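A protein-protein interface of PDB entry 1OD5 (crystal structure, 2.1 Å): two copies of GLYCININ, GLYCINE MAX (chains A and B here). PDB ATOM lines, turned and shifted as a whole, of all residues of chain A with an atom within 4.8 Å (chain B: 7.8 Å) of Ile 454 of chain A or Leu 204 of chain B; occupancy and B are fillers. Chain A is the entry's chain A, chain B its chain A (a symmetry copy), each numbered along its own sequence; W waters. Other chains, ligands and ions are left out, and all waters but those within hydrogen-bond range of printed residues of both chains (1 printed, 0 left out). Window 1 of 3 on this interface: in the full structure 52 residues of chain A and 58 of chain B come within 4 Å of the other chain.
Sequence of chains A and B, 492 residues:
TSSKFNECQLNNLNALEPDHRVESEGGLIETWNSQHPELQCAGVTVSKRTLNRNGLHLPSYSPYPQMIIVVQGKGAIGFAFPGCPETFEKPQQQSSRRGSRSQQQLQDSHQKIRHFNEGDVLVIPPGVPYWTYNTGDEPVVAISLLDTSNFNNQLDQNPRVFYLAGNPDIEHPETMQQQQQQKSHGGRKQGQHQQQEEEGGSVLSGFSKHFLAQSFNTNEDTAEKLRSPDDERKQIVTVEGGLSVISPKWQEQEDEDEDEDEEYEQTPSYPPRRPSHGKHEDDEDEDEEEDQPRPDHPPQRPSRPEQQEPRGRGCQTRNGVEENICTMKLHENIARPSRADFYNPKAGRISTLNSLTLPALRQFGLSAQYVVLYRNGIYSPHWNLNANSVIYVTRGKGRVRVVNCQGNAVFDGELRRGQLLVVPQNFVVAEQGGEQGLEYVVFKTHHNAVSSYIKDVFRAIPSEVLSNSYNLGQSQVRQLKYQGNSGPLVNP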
ATOM      1  N   PRO A 381      30.628  -9.047  10.126  1.00  0.00           N
ATOM      2  CA  PRO A 381      29.717  -7.993   9.668  1.00  0.00           C
ATOM      3  C   PRO A 381      29.438  -6.884  10.677  1.00  0.00           C
ATOM      4  O   PRO A 381      29.063  -7.154  11.814  1.00  0.00           O
ATOM      5  CB  PRO A 381      28.474  -8.757   9.271  1.00  0.00           C
ATOM      6  CG  PRO A 381      29.004 -10.079   8.754  1.00  0.00           C
ATOM      7  CD  PRO A 381      30.108 -10.365   9.743  1.00  0.00           C
ATOM      8  N   TRP A 383      28.512  -2.197  11.169  1.00  0.00           N
ATOM      9  CA  TRP A 383      28.123  -0.934  10.555  1.00  0.00           C
ATOM     10  C   TRP A 383      28.410   0.207  11.523  1.00  0.00           C
ATOM     11  O   TRP A 383      28.488  -0.031  12.728  1.00  0.00           O
ATOM     12  CB  TRP A 383      26.629  -0.873  10.234  1.00  0.00           C
ATOM     13  CG  TRP A 383      25.649  -0.815  11.411  1.00  0.00           C
ATOM     14  CD1 TRP A 383      25.123   0.374  11.853  1.00  0.00           C
ATOM     15  CD2 TRP A 383      25.129  -1.895  12.079  1.00  0.00           C
ATOM     16  NE1 TRP A 383      24.267   0.046  12.783  1.00  0.00           N
ATOM     17  CE2 TRP A 383      24.239  -1.276  12.953  1.00  0.00           C
ATOM     18  CE3 TRP A 383      25.264  -3.278  12.076  1.00  0.00           C
ATOM     19  CZ2 TRP A 383      23.464  -2.020  13.827  1.00  0.00           C
ATOM     20  CZ3 TRP A 383      24.491  -4.035  12.950  1.00  0.00           C
ATOM     21  CH2 TRP A 383      23.601  -3.409  13.815  1.00  0.00           C
ATOM     22  N   VAL A 428      26.366  -2.179   6.065  1.00  0.00           N
ATOM     23  CA  VAL A 428      27.052  -3.281   6.706  1.00  0.00           C
ATOM     24  C   VAL A 428      28.289  -3.743   5.956  1.00  0.00           C
ATOM     25  O   VAL A 428      28.165  -4.218   4.837  1.00  0.00           O
ATOM     26  CB  VAL A 428      25.997  -4.382   6.857  1.00  0.00           C
ATOM     27  CG1 VAL A 428      26.502  -5.577   7.606  1.00  0.00           C
ATOM     28  CG2 VAL A 428      24.875  -3.852   7.681  1.00  0.00           C
ATOM     29  N   SER A 452      28.704  -1.204  15.521  1.00  0.00           N
ATOM     30  CA  SER A 452      28.063  -2.307  16.178  1.00  0.00           C
ATOM     31  C   SER A 452      28.336  -3.537  15.347  1.00  0.00           C
ATOM     32  O   SER A 452      28.459  -3.378  14.138  1.00  0.00           O
ATOM     33  CB  SER A 452      26.608  -2.037  16.247  1.00  0.00           C
ATOM     34  OG  SER A 452      26.031  -3.105  16.946  1.00  0.00           O
ATOM     35  N   TYR A 453      28.543  -4.736  15.889  1.00  0.00           N
ATOM     36  CA  TYR A 453      28.770  -5.892  15.045  1.00  0.00           C
ATOM     37  C   TYR A 453      27.617  -6.837  15.304  1.00  0.00           C
ATOM     38  O   TYR A 453      27.107  -6.901  16.431  1.00  0.00           O
ATOM     39  CB  TYR A 453      30.115  -6.540  15.331  1.00  0.00           C
ATOM     40  CG  TYR A 453      30.458  -6.905  16.755  1.00  0.00           C
ATOM     41  CD1 TYR A 453      30.484  -8.250  17.092  1.00  0.00           C
ATOM     42  CD2 TYR A 453      30.767  -5.930  17.716  1.00  0.00           C
ATOM     43  CE1 TYR A 453      30.819  -8.645  18.385  1.00  0.00           C
ATOM     44  CE2 TYR A 453      31.100  -6.316  19.021  1.00  0.00           C
ATOM     45  CZ  TYR A 453      31.119  -7.671  19.323  1.00  0.00           C
ATOM     46  OH  TYR A 453      31.444  -8.095  20.575  1.00  0.00           O
ATOM     47  N   ILE A 454      27.134  -7.539  14.271  1.00  0.00           N
ATOM     48  CA  ILE A 454      25.991  -8.426  14.406  1.00  0.00           C
ATOM     49  C   ILE A 454      26.058  -9.550  15.417  1.00  0.00           C
ATOM     50  O   ILE A 454      24.996  -9.857  15.936  1.00  0.00           O
ATOM     51  CB  ILE A 454      25.667  -8.951  13.002  1.00  0.00           C
ATOM     52  CG1 ILE A 454      25.105  -7.752  12.261  1.00  0.00           C
ATOM     53  CG2 ILE A 454      24.575  -9.999  12.947  1.00  0.00           C
ATOM     54  CD1 ILE A 454      25.121  -7.922  10.742  1.00  0.00           C
ATOM     55  N   LYS A 455      27.189 -10.179  15.748  1.00  0.00           N
ATOM     56  CA  LYS A 455      27.239 -11.249  16.763  1.00  0.00           C
ATOM     57  C   LYS A 455      26.716 -10.716  18.112  1.00  0.00           C
ATOM     58  O   LYS A 455      25.856 -11.278  18.801  1.00  0.00           O
ATOM     59  CB  LYS A 455      28.676 -11.738  16.962  1.00  0.00           C
ATOM     60  CG  LYS A 455      29.380 -12.332  15.747  1.00  0.00           C
ATOM     61  CD  LYS A 455      30.943 -12.221  15.768  1.00  0.00           C
ATOM     62  CE  LYS A 455      31.707 -13.152  16.710  1.00  0.00           C
ATOM     63  NZ  LYS A 455      31.682 -14.523  16.214  1.00  0.00           N
ATOM     64  N   ASP A 456      27.161  -9.488  18.348  1.00  0.00           N
ATOM     65  CA  ASP A 456      26.809  -8.768  19.534  1.00  0.00           C
ATOM     66  C   ASP A 456      25.359  -8.406  19.510  1.00  0.00           C
ATOM     67  O   ASP A 456      24.787  -8.413  20.600  1.00  0.00           O
ATOM     68  CB  ASP A 456      27.642  -7.494  19.660  1.00  0.00           C
ATOM     69  CG  ASP A 456      27.451  -6.748  20.973  1.00  0.00           C
ATOM     70  OD1 ASP A 456      27.769  -7.299  22.028  1.00  0.00           O
ATOM     71  OD2 ASP A 456      26.941  -5.624  20.946  1.00  0.00           O
ATOM     72  N   VAL A 457      24.695  -8.065  18.392  1.00  0.00           N
ATOM     73  CA  VAL A 457      23.288  -7.729  18.540  1.00  0.00           C
ATOM     74  C   VAL A 457      22.481  -9.019  18.712  1.00  0.00           C
ATOM     75  O   VAL A 457      21.407  -8.970  19.314  1.00  0.00           O
ATOM     76  CB  VAL A 457      22.729  -6.792  17.318  1.00  0.00           C
ATOM     77  CG1 VAL A 457      23.917  -6.096  16.652  1.00  0.00           C
ATOM     78  CG2 VAL A 457      21.868  -7.528  16.325  1.00  0.00           C
ATOM     79  N   PHE A 458      22.984 -10.191  18.304  1.00  0.00           N
ATOM     80  CA  PHE A 458      22.252 -11.430  18.486  1.00  0.00           C
ATOM     81  C   PHE A 458      22.184 -11.696  19.983  1.00  0.00           C
ATOM     82  O   PHE A 458      21.184 -12.179  20.500  1.00  0.00           O
ATOM     83  CB  PHE A 458      22.939 -12.657  17.823  1.00  0.00           C
ATOM     84  CG  PHE A 458      22.938 -12.764  16.291  1.00  0.00           C
ATOM     85  CD1 PHE A 458      23.972 -13.484  15.674  1.00  0.00           C
ATOM     86  CD2 PHE A 458      21.946 -12.147  15.515  1.00  0.00           C
ATOM     87  CE1 PHE A 458      24.011 -13.575  14.280  1.00  0.00           C
ATOM     88  CE2 PHE A 458      21.998 -12.248  14.118  1.00  0.00           C
ATOM     89  CZ  PHE A 458      23.030 -12.961  13.504  1.00  0.00           C
ATOM     90  N   TYR A 470      14.319 -15.638  11.978  1.00  0.00           N
ATOM     91  CA  TYR A 470      15.025 -16.439  10.989  1.00  0.00           C
ATOM     92  C   TYR A 470      14.570 -17.883  10.898  1.00  0.00           C
ATOM     93  O   TYR A 470      15.283 -18.710  10.324  1.00  0.00           O
ATOM     94  CB  TYR A 470      16.521 -16.443  11.298  1.00  0.00           C
ATOM     95  CG  TYR A 470      17.161 -15.067  11.429  1.00  0.00           C
ATOM     96  CD1 TYR A 470      17.367 -14.517  12.701  1.00  0.00           C
ATOM     97  CD2 TYR A 470      17.556 -14.354  10.303  1.00  0.00           C
ATOM     98  CE1 TYR A 470      17.959 -13.263  12.856  1.00  0.00           C
ATOM     99  CE2 TYR A 470      18.152 -13.106  10.443  1.00  0.00           C
ATOM    100  CZ  TYR A 470      18.345 -12.576  11.725  1.00  0.00           C
ATOM    101  OH  TYR A 470      18.937 -11.354  11.880  1.00  0.00           O
ATOM    102  N   TYR B  61      17.105  -0.858  11.756  1.00  0.00           N
ATOM    103  CA  TYR B  61      17.676   0.420  12.158  1.00  0.00           C
ATOM    104  C   TYR B  61      17.634   1.404  10.989  1.00  0.00           C
ATOM    105  O   TYR B  61      17.470   1.008   9.833  1.00  0.00           O
ATOM    106  CB  TYR B  61      19.105   0.258  12.620  1.00  0.00           C
ATOM    107  CG  TYR B  61      20.092  -0.386  11.685  1.00  0.00           C
ATOM    108  CD1 TYR B  61      20.241  -1.769  11.631  1.00  0.00           C
ATOM    109  CD2 TYR B  61      20.887   0.439  10.914  1.00  0.00           C
ATOM    110  CE1 TYR B  61      21.212  -2.330  10.794  1.00  0.00           C
ATOM    111  CE2 TYR B  61      21.855  -0.114  10.083  1.00  0.00           C
ATOM    112  CZ  TYR B  61      22.008  -1.482  10.034  1.00  0.00           C
ATOM    113  OH  TYR B  61      22.979  -1.980   9.231  1.00  0.00           O
ATOM    114  N   PRO B 129      19.424  -0.967  16.380  1.00  0.00           N
ATOM    115  CA  PRO B 129      18.409  -1.969  16.057  1.00  0.00           C
ATOM    116  C   PRO B 129      17.294  -2.044  17.090  1.00  0.00           C
ATOM    117  O   PRO B 129      17.549  -1.938  18.293  1.00  0.00           O
ATOM    118  CB  PRO B 129      19.139  -3.278  15.973  1.00  0.00           C
ATOM    119  CG  PRO B 129      20.568  -2.902  15.816  1.00  0.00           C
ATOM    120  CD  PRO B 129      20.742  -1.580  16.547  1.00  0.00           C
ATOM    121  N   TYR B 163      16.955  -3.739   7.531  1.00  0.00           N
ATOM    122  CA  TYR B 163      16.424  -4.879   8.260  1.00  0.00           C
ATOM    123  C   TYR B 163      17.466  -5.947   8.523  1.00  0.00           C
ATOM    124  O   TYR B 163      18.284  -6.217   7.649  1.00  0.00           O
ATOM    125  CB  TYR B 163      15.274  -5.503   7.489  1.00  0.00           C
ATOM    126  CG  TYR B 163      13.991  -4.764   7.790  1.00  0.00           C
ATOM    127  CD1 TYR B 163      13.575  -3.723   6.964  1.00  0.00           C
ATOM    128  CD2 TYR B 163      13.229  -5.120   8.895  1.00  0.00           C
ATOM    129  CE1 TYR B 163      12.393  -3.052   7.251  1.00  0.00           C
ATOM    130  CE2 TYR B 163      12.042  -4.445   9.183  1.00  0.00           C
ATOM    131  CZ  TYR B 163      11.644  -3.419   8.354  1.00  0.00           C
ATOM    132  OH  TYR B 163      10.473  -2.777   8.611  1.00  0.00           O
ATOM    133  N   LEU B 164      17.485  -6.533   9.735  1.00  0.00           N
ATOM    134  CA  LEU B 164      18.443  -7.577  10.074  1.00  0.00           C
ATOM    135  C   LEU B 164      17.878  -8.952   9.787  1.00  0.00           C
ATOM    136  O   LEU B 164      18.632  -9.917   9.738  1.00  0.00           O
ATOM    137  CB  LEU B 164      18.838  -7.438  11.545  1.00  0.00           C
ATOM    138  CG  LEU B 164      19.629  -6.168  11.882  1.00  0.00           C
ATOM    139  CD1 LEU B 164      19.593  -5.947  13.373  1.00  0.00           C
ATOM    140  CD2 LEU B 164      21.065  -6.289  11.402  1.00  0.00           C
ATOM    141  N   ALA B 165      16.570  -9.066   9.545  1.00  0.00           N
ATOM    142  CA  ALA B 165      15.895 -10.321   9.218  1.00  0.00           C
ATOM    143  C   ALA B 165      14.754 -10.107   8.221  1.00  0.00           C
ATOM    144  O   ALA B 165      14.375  -8.966   7.960  1.00  0.00           O
ATOM    145  CB  ALA B 165      15.281 -10.934  10.440  1.00  0.00           C
ATOM    146  N   GLY B 166      14.192 -11.173   7.621  1.00  0.00           N
ATOM    147  CA  GLY B 166      13.073 -11.102   6.658  1.00  0.00           C
ATOM    148  C   GLY B 166      13.325 -10.533   5.257  1.00  0.00           C
ATOM    149  O   GLY B 166      14.463 -10.293   4.854  1.00  0.00           O
ATOM    150  N   GLY B 201      15.707  -7.133   0.392  1.00  0.00           N
ATOM    151  CA  GLY B 201      16.117  -8.128   1.369  1.00  0.00           C
ATOM    152  C   GLY B 201      16.672  -7.499   2.642  1.00  0.00           C
ATOM    153  O   GLY B 201      16.666  -6.282   2.817  1.00  0.00           O
ATOM    154  N   SER B 202      17.094  -8.367   3.571  1.00  0.00           N
ATOM    155  CA  SER B 202      17.680  -7.919   4.834  1.00  0.00           C
ATOM    156  C   SER B 202      19.152  -7.637   4.592  1.00  0.00           C
ATOM    157  O   SER B 202      19.666  -8.063   3.558  1.00  0.00           O
ATOM    158  CB  SER B 202      17.549  -9.003   5.846  1.00  0.00           C
ATOM    159  OG  SER B 202      18.302 -10.123   5.412  1.00  0.00           O
ATOM    160  N   VAL B 203      19.938  -7.032   5.485  1.00  0.00           N
ATOM    161  CA  VAL B 203      21.340  -6.763   5.184  1.00  0.00           C
ATOM    162  C   VAL B 203      22.201  -8.012   5.200  1.00  0.00           C
ATOM    163  O   VAL B 203      23.296  -8.020   4.659  1.00  0.00           O
ATOM    164  CB  VAL B 203      21.895  -5.721   6.187  1.00  0.00           C
ATOM    165  CG1 VAL B 203      20.954  -4.551   6.225  1.00  0.00           C
ATOM    166  CG2 VAL B 203      21.995  -6.275   7.606  1.00  0.00           C
ATOM    167  N   LEU B 204      21.740  -9.104   5.799  1.00  0.00           N
ATOM    168  CA  LEU B 204      22.510 -10.327   5.852  1.00  0.00           C
ATOM    169  C   LEU B 204      22.420 -11.187   4.604  1.00  0.00           C
ATOM    170  O   LEU B 204      23.285 -12.028   4.393  1.00  0.00           O
ATOM    171  CB  LEU B 204      22.059 -11.101   7.075  1.00  0.00           C
ATOM    172  CG  LEU B 204      22.582 -10.625   8.424  1.00  0.00           C
ATOM    173  CD1 LEU B 204      22.118 -11.613   9.488  1.00  0.00           C
ATOM    174  CD2 LEU B 204      24.109 -10.597   8.432  1.00  0.00           C
ATOM    175  N   SER B 205      21.380 -10.967   3.766  1.00  0.00           N
ATOM    176  CA  SER B 205      21.160 -11.680   2.507  1.00  0.00           C
ATOM    177  C   SER B 205      22.194 -11.313   1.437  1.00  0.00           C
ATOM    178  O   SER B 205      22.461 -12.080   0.514  1.00  0.00           O
ATOM    179  CB  SER B 205      19.762 -11.361   1.997  1.00  0.00           C
ATOM    180  OG  SER B 205      19.667 -10.070   1.403  1.00  0.00           O
ATOM    181  N   GLY B 206      22.818 -10.140   1.581  1.00  0.00           N
ATOM    182  CA  GLY B 206      23.850  -9.644   0.677  1.00  0.00           C
ATOM    183  C   GLY B 206      25.174 -10.337   0.927  1.00  0.00           C
ATOM    184  O   GLY B 206      26.161 -10.027   0.276  1.00  0.00           O
ATOM    185  N   PHE B 207      25.240 -11.265   1.893  1.00  0.00           N
ATOM    186  CA  PHE B 207      26.450 -12.014   2.225  1.00  0.00           C
ATOM    187  C   PHE B 207      26.189 -13.461   1.847  1.00  0.00           C
ATOM    188  O   PHE B 207      25.048 -13.883   2.012  1.00  0.00           O
ATOM    189  CB  PHE B 207      26.752 -11.953   3.750  1.00  0.00           C
ATOM    190  CG  PHE B 207      27.318 -10.636   4.241  1.00  0.00           C
ATOM    191  CD1 PHE B 207      28.630 -10.283   3.904  1.00  0.00           C
ATOM    192  CD2 PHE B 207      26.522  -9.766   4.976  1.00  0.00           C
ATOM    193  CE1 PHE B 207      29.132  -9.047   4.301  1.00  0.00           C
ATOM    194  CE2 PHE B 207      27.039  -8.527   5.369  1.00  0.00           C
ATOM    195  CZ  PHE B 207      28.338  -8.167   5.030  1.00  0.00           C
ATOM    196  N   SER B 208      27.156 -14.265   1.381  1.00  0.00           N
ATOM    197  CA  SER B 208      26.885 -15.666   1.048  1.00  0.00           C
ATOM    198  C   SER B 208      26.648 -16.553   2.254  1.00  0.00           C
ATOM    199  O   SER B 208      27.136 -16.181   3.320  1.00  0.00           O
ATOM    200  CB  SER B 208      28.033 -16.255   0.294  1.00  0.00           C
ATOM    201  OG  SER B 208      29.254 -16.066   0.982  1.00  0.00           O
ATOM    202  N   LYS B 209      25.983 -17.725   2.213  1.00  0.00           N
ATOM    203  CA  LYS B 209      25.790 -18.544   3.420  1.00  0.00           C
ATOM    204  C   LYS B 209      27.109 -19.057   3.999  1.00  0.00           C
ATOM    205  O   LYS B 209      27.222 -19.219   5.206  1.00  0.00           O
ATOM    206  CB  LYS B 209      24.858 -19.742   3.115  1.00  0.00           C
ATOM    207  CG  LYS B 209      25.513 -20.778   2.221  1.00  0.00           C
ATOM    208  CD  LYS B 209      24.613 -21.835   1.578  1.00  0.00           C
ATOM    209  CE  LYS B 209      25.514 -22.924   0.936  1.00  0.00           C
ATOM    210  NZ  LYS B 209      26.544 -22.423   0.013  1.00  0.00           N
ATOM    211  N   PHE B 211      30.309 -17.478   4.029  1.00  0.00           N
ATOM    212  CA  PHE B 211      31.010 -16.467   4.788  1.00  0.00           C
ATOM    213  C   PHE B 211      30.301 -16.193   6.102  1.00  0.00           C
ATOM    214  O   PHE B 211      30.936 -15.895   7.096  1.00  0.00           O
ATOM    215  CB  PHE B 211      31.076 -15.186   3.961  1.00  0.00           C
ATOM    216  CG  PHE B 211      31.733 -14.007   4.665  1.00  0.00           C
ATOM    217  CD1 PHE B 211      30.953 -12.917   5.047  1.00  0.00           C
ATOM    218  CD2 PHE B 211      33.099 -14.046   4.950  1.00  0.00           C
ATOM    219  CE1 PHE B 211      31.559 -11.860   5.728  1.00  0.00           C
ATOM    220  CE2 PHE B 211      33.682 -12.983   5.626  1.00  0.00           C
ATOM    221  CZ  PHE B 211      32.919 -11.894   6.017  1.00  0.00           C
ATOM    222  N   LEU B 212      28.976 -16.243   6.078  1.00  0.00           N
ATOM    223  CA  LEU B 212      28.176 -15.995   7.247  1.00  0.00           C
ATOM    224  C   LEU B 212      28.422 -17.157   8.189  1.00  0.00           C
ATOM    225  O   LEU B 212      28.481 -16.937   9.391  1.00  0.00           O
ATOM    226  CB  LEU B 212      26.743 -15.928   6.831  1.00  0.00           C
ATOM    227  CG  LEU B 212      25.900 -14.707   7.134  1.00  0.00           C
ATOM    228  CD1 LEU B 212      26.668 -13.417   6.886  1.00  0.00           C
ATOM    229  CD2 LEU B 212      24.644 -14.819   6.310  1.00  0.00           C
ATOM    230  N   PHE B 216      30.219 -16.128  11.941  1.00  0.00           N
ATOM    231  CA  PHE B 216      29.515 -16.334  13.191  1.00  0.00           C
ATOM    232  C   PHE B 216      29.764 -17.705  13.787  1.00  0.00           C
ATOM    233  O   PHE B 216      29.050 -18.114  14.699  1.00  0.00           O
ATOM    234  CB  PHE B 216      28.000 -16.196  13.007  1.00  0.00           C
ATOM    235  CG  PHE B 216      27.504 -14.921  12.365  1.00  0.00           C
ATOM    236  CD1 PHE B 216      26.368 -14.981  11.565  1.00  0.00           C
ATOM    237  CD2 PHE B 216      28.162 -13.702  12.554  1.00  0.00           C
ATOM    238  CE1 PHE B 216      25.884 -13.829  10.950  1.00  0.00           C
ATOM    239  CE2 PHE B 216      27.674 -12.553  11.936  1.00  0.00           C
ATOM    240  CZ  PHE B 216      26.534 -12.617  11.135  1.00  0.00           C
ATOM    241  N   ALA B 223      23.600 -20.624   8.766  1.00  0.00           N
ATOM    242  CA  ALA B 223      24.042 -19.468   7.992  1.00  0.00           C
ATOM    243  C   ALA B 223      23.100 -19.140   6.832  1.00  0.00           C
ATOM    244  O   ALA B 223      22.886 -17.983   6.463  1.00  0.00           O
ATOM    245  CB  ALA B 223      25.418 -19.757   7.458  1.00  0.00           C
ATOM    246  N   GLU B 224      22.498 -20.200   6.290  1.00  0.00           N
ATOM    247  CA  GLU B 224      21.550 -20.143   5.196  1.00  0.00           C
ATOM    248  C   GLU B 224      20.234 -19.552   5.660  1.00  0.00           C
ATOM    249  O   GLU B 224      19.682 -18.735   4.935  1.00  0.00           O
ATOM    250  CB  GLU B 224      21.353 -21.538   4.689  1.00  0.00           C
ATOM    251  CG  GLU B 224      20.266 -21.823   3.661  1.00  0.00           C
ATOM    252  CD  GLU B 224      19.803 -23.279   3.801  1.00  0.00           C
ATOM    253  OE1 GLU B 224      18.744 -23.517   4.405  1.00  0.00           O
ATOM    254  OE2 GLU B 224      20.522 -24.173   3.336  1.00  0.00           O
ATOM    255  N   LYS B 225      19.703 -19.918   6.832  1.00  0.00           N
ATOM    256  CA  LYS B 225      18.452 -19.365   7.332  1.00  0.00           C
ATOM    257  C   LYS B 225      18.533 -17.912   7.758  1.00  0.00           C
ATOM    258  O   LYS B 225      17.525 -17.218   7.896  1.00  0.00           O
ATOM    259  CB  LYS B 225      17.997 -20.160   8.500  1.00  0.00           C
ATOM    260  CG  LYS B 225      17.541 -21.488   7.993  1.00  0.00           C
ATOM    261  CD  LYS B 225      16.904 -22.256   9.111  1.00  0.00           C
ATOM    262  CE  LYS B 225      15.937 -23.236   8.477  1.00  0.00           C
ATOM    263  NZ  LYS B 225      14.865 -22.496   7.819  1.00  0.00           N
ATOM    264  N   LEU B 226      19.760 -17.417   7.940  1.00  0.00           N
ATOM    265  CA  LEU B 226      19.959 -16.036   8.354  1.00  0.00           C
ATOM    266  C   LEU B 226      19.805 -15.087   7.175  1.00  0.00           C
ATOM    267  O   LEU B 226      19.663 -13.873   7.349  1.00  0.00           O
ATOM    268  CB  LEU B 226      21.350 -15.866   8.986  1.00  0.00           C
ATOM    269  CG  LEU B 226      21.701 -16.657  10.237  1.00  0.00           C
ATOM    270  CD1 LEU B 226      23.114 -16.337  10.601  1.00  0.00           C
ATOM    271  CD2 LEU B 226      20.773 -16.319  11.378  1.00  0.00           C
ATOM    272  N   ARG B 227      19.803 -15.652   5.956  1.00  0.00           N
ATOM    273  CA  ARG B 227      19.644 -14.874   4.744  1.00  0.00           C
ATOM    274  C   ARG B 227      18.188 -14.638   4.381  1.00  0.00           C
ATOM    275  O   ARG B 227      17.875 -13.796   3.547  1.00  0.00           O
ATOM    276  CB  ARG B 227      20.345 -15.597   3.645  1.00  0.00           C
ATOM    277  CG  ARG B 227      21.817 -15.753   3.974  1.00  0.00           C
ATOM    278  CD  ARG B 227      22.581 -16.418   2.858  1.00  0.00           C
ATOM    279  NE  ARG B 227      22.868 -15.522   1.736  1.00  0.00           N
ATOM    280  CZ  ARG B 227      22.259 -15.580   0.541  1.00  0.00           C
ATOM    281  NH1 ARG B 227      21.298 -16.464   0.290  1.00  0.00           N
ATOM    282  NH2 ARG B 227      22.665 -14.763  -0.434  1.00  0.00           N
ATOM    283  N   SER B 228      17.285 -15.354   5.059  1.00  0.00           N
ATOM    284  CA  SER B 228      15.834 -15.315   4.877  1.00  0.00           C
ATOM    285  C   SER B 228      15.339 -15.695   3.477  1.00  0.00           C
ATOM    286  O   SER B 228      14.510 -14.998   2.880  1.00  0.00           O
ATOM    287  CB  SER B 228      15.292 -13.933   5.253  1.00  0.00           C
ATOM    288  OG  SER B 228      15.460 -13.779   6.650  1.00  0.00           O
HETATM  289  O   HOH W   1      14.840 -18.143   7.008  1.00  0.00           O
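Water W1 lies within hydrogen-bond range of the backbone carbonyl oxygen (O) of Lys 225 of chain B and the backbone carbonyl oxygen (O) of Tyr 470 of chain A.
No position is printed for both chains.
Of the 15 pairs that touch across the chains among the printed residues, none has its exchanged pair printed and touching as well.
The backbone NH (N) of Ser 452 of chain A sits at hydrogen-bond distance from the backbone carbonyl oxygen (O) of Trp 383 of chain A (3.0 Å).
O of Tyr 163 of chain B lies within hydrogen-bond range of N of Val 203 of chain B, at 2.8 Å.
The backbone NH of Ile 454 of chain A lies within hydrogen-bond range of the backbone carbonyl oxygen of Pro 381 of chain A, 3.1 Å away.
The backbone carbonyl oxygen (O) of Phe 207 of chain B is in hydrogen-bond range of the guanidinium group (NE) of Arg 227 of chain B (2.7 Å).
Phe 216 of chain B touches Pro 381 of chain A (CE2 to CD, 3.9 Å).
Trp 383 of chain A touches Tyr 61 of chain B (CD2 to OH, 3.6 Å).
Pro 129 of chain B touches Trp 383 of chain A (CG to CZ2, 3.6 Å).
Val 428 of chain A touches Tyr 61 of chain B (CG2 to OH, 3.1 Å).
CE2 of Phe 207 of chain B touches CG1 of Val 428 of chain A (3.7 Å).
Leu 204 of chain B touches Ile 454 of chain A.
Phe 216 of chain B touches Lys 455 of chain A (CD2 to CG, 3.7 Å).
Phe 216 of chain B touches Phe 458 of chain A (CE1 to CE1, 3.8 Å).
Tyr 470 of chain A touches Leu 204 of chain B (OH to CD1, 3.99 Å).
Tyr 470 of chain A touches Leu 226 of chain B.
Of the 24 printed residues of chain B, 10 touch a printed residue of chain A.
Hydrophobic or aromatic side chains of chain B that line the printed part of chain A: Tyr 61, Pro 129, Leu 164, Ala 165, Val 203, Leu 204, Phe 207, Phe 216 and Leu 226.
Of the 11 printed residues of chain A, 7 touch a printed residue of chain B.
Printed residues of chain A that touch a printed residue of chain B: Pro 381, Trp 383, Val 428, Ile 454, Lys 455, Phe 458 and Tyr 470.
Hydrophobic or aromatic side chains of chain A that line the printed part of chain B: Pro 381, Trp 383, Val 428, Ile 454, Phe 458 and Tyr 470.
Among the printed residues, no Asp or Glu carboxylate lies within 4 Å of a Lys or Arg side-chain nitrogen of the other chain.
Of chain B, only Leu 204 (3.7 Å) and Phe 216 (3.7 Å) come within 4 Å of Ile 454 of chain A.
Of the printed residues of chain A, Leu 204 of chain B touches Ile 454 (3.7 Å) and Tyr 470 (3.99 Å).
Printed residues of chain A within 4 Å of Lys 225 of chain B: Tyr 470.
Printed residues of chain B within 4 Å of Trp 383 of chain A: Tyr 61 (3.6 Å) and Pro 129 (3.6 Å).
Of the printed residues of chain A, Val 203 of chain B touches Val 428 (3.8 Å).
Of the printed residues of chain A, Phe 207 of chain B touches Val 428 (3.7 Å).
The nearest residue of chain B that does not touch Ile 454 of chain A is Leu 164 of chain B (4.4 Å).
The nearest printed residue of chain A that does not touch Leu 204 of chain B is Phe 458 of chain A (4.3 Å).
OH of Tyr 470 of chain A is in hydrogen-bond range of O of Leu 164 of chain B, 2.6 Å away.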
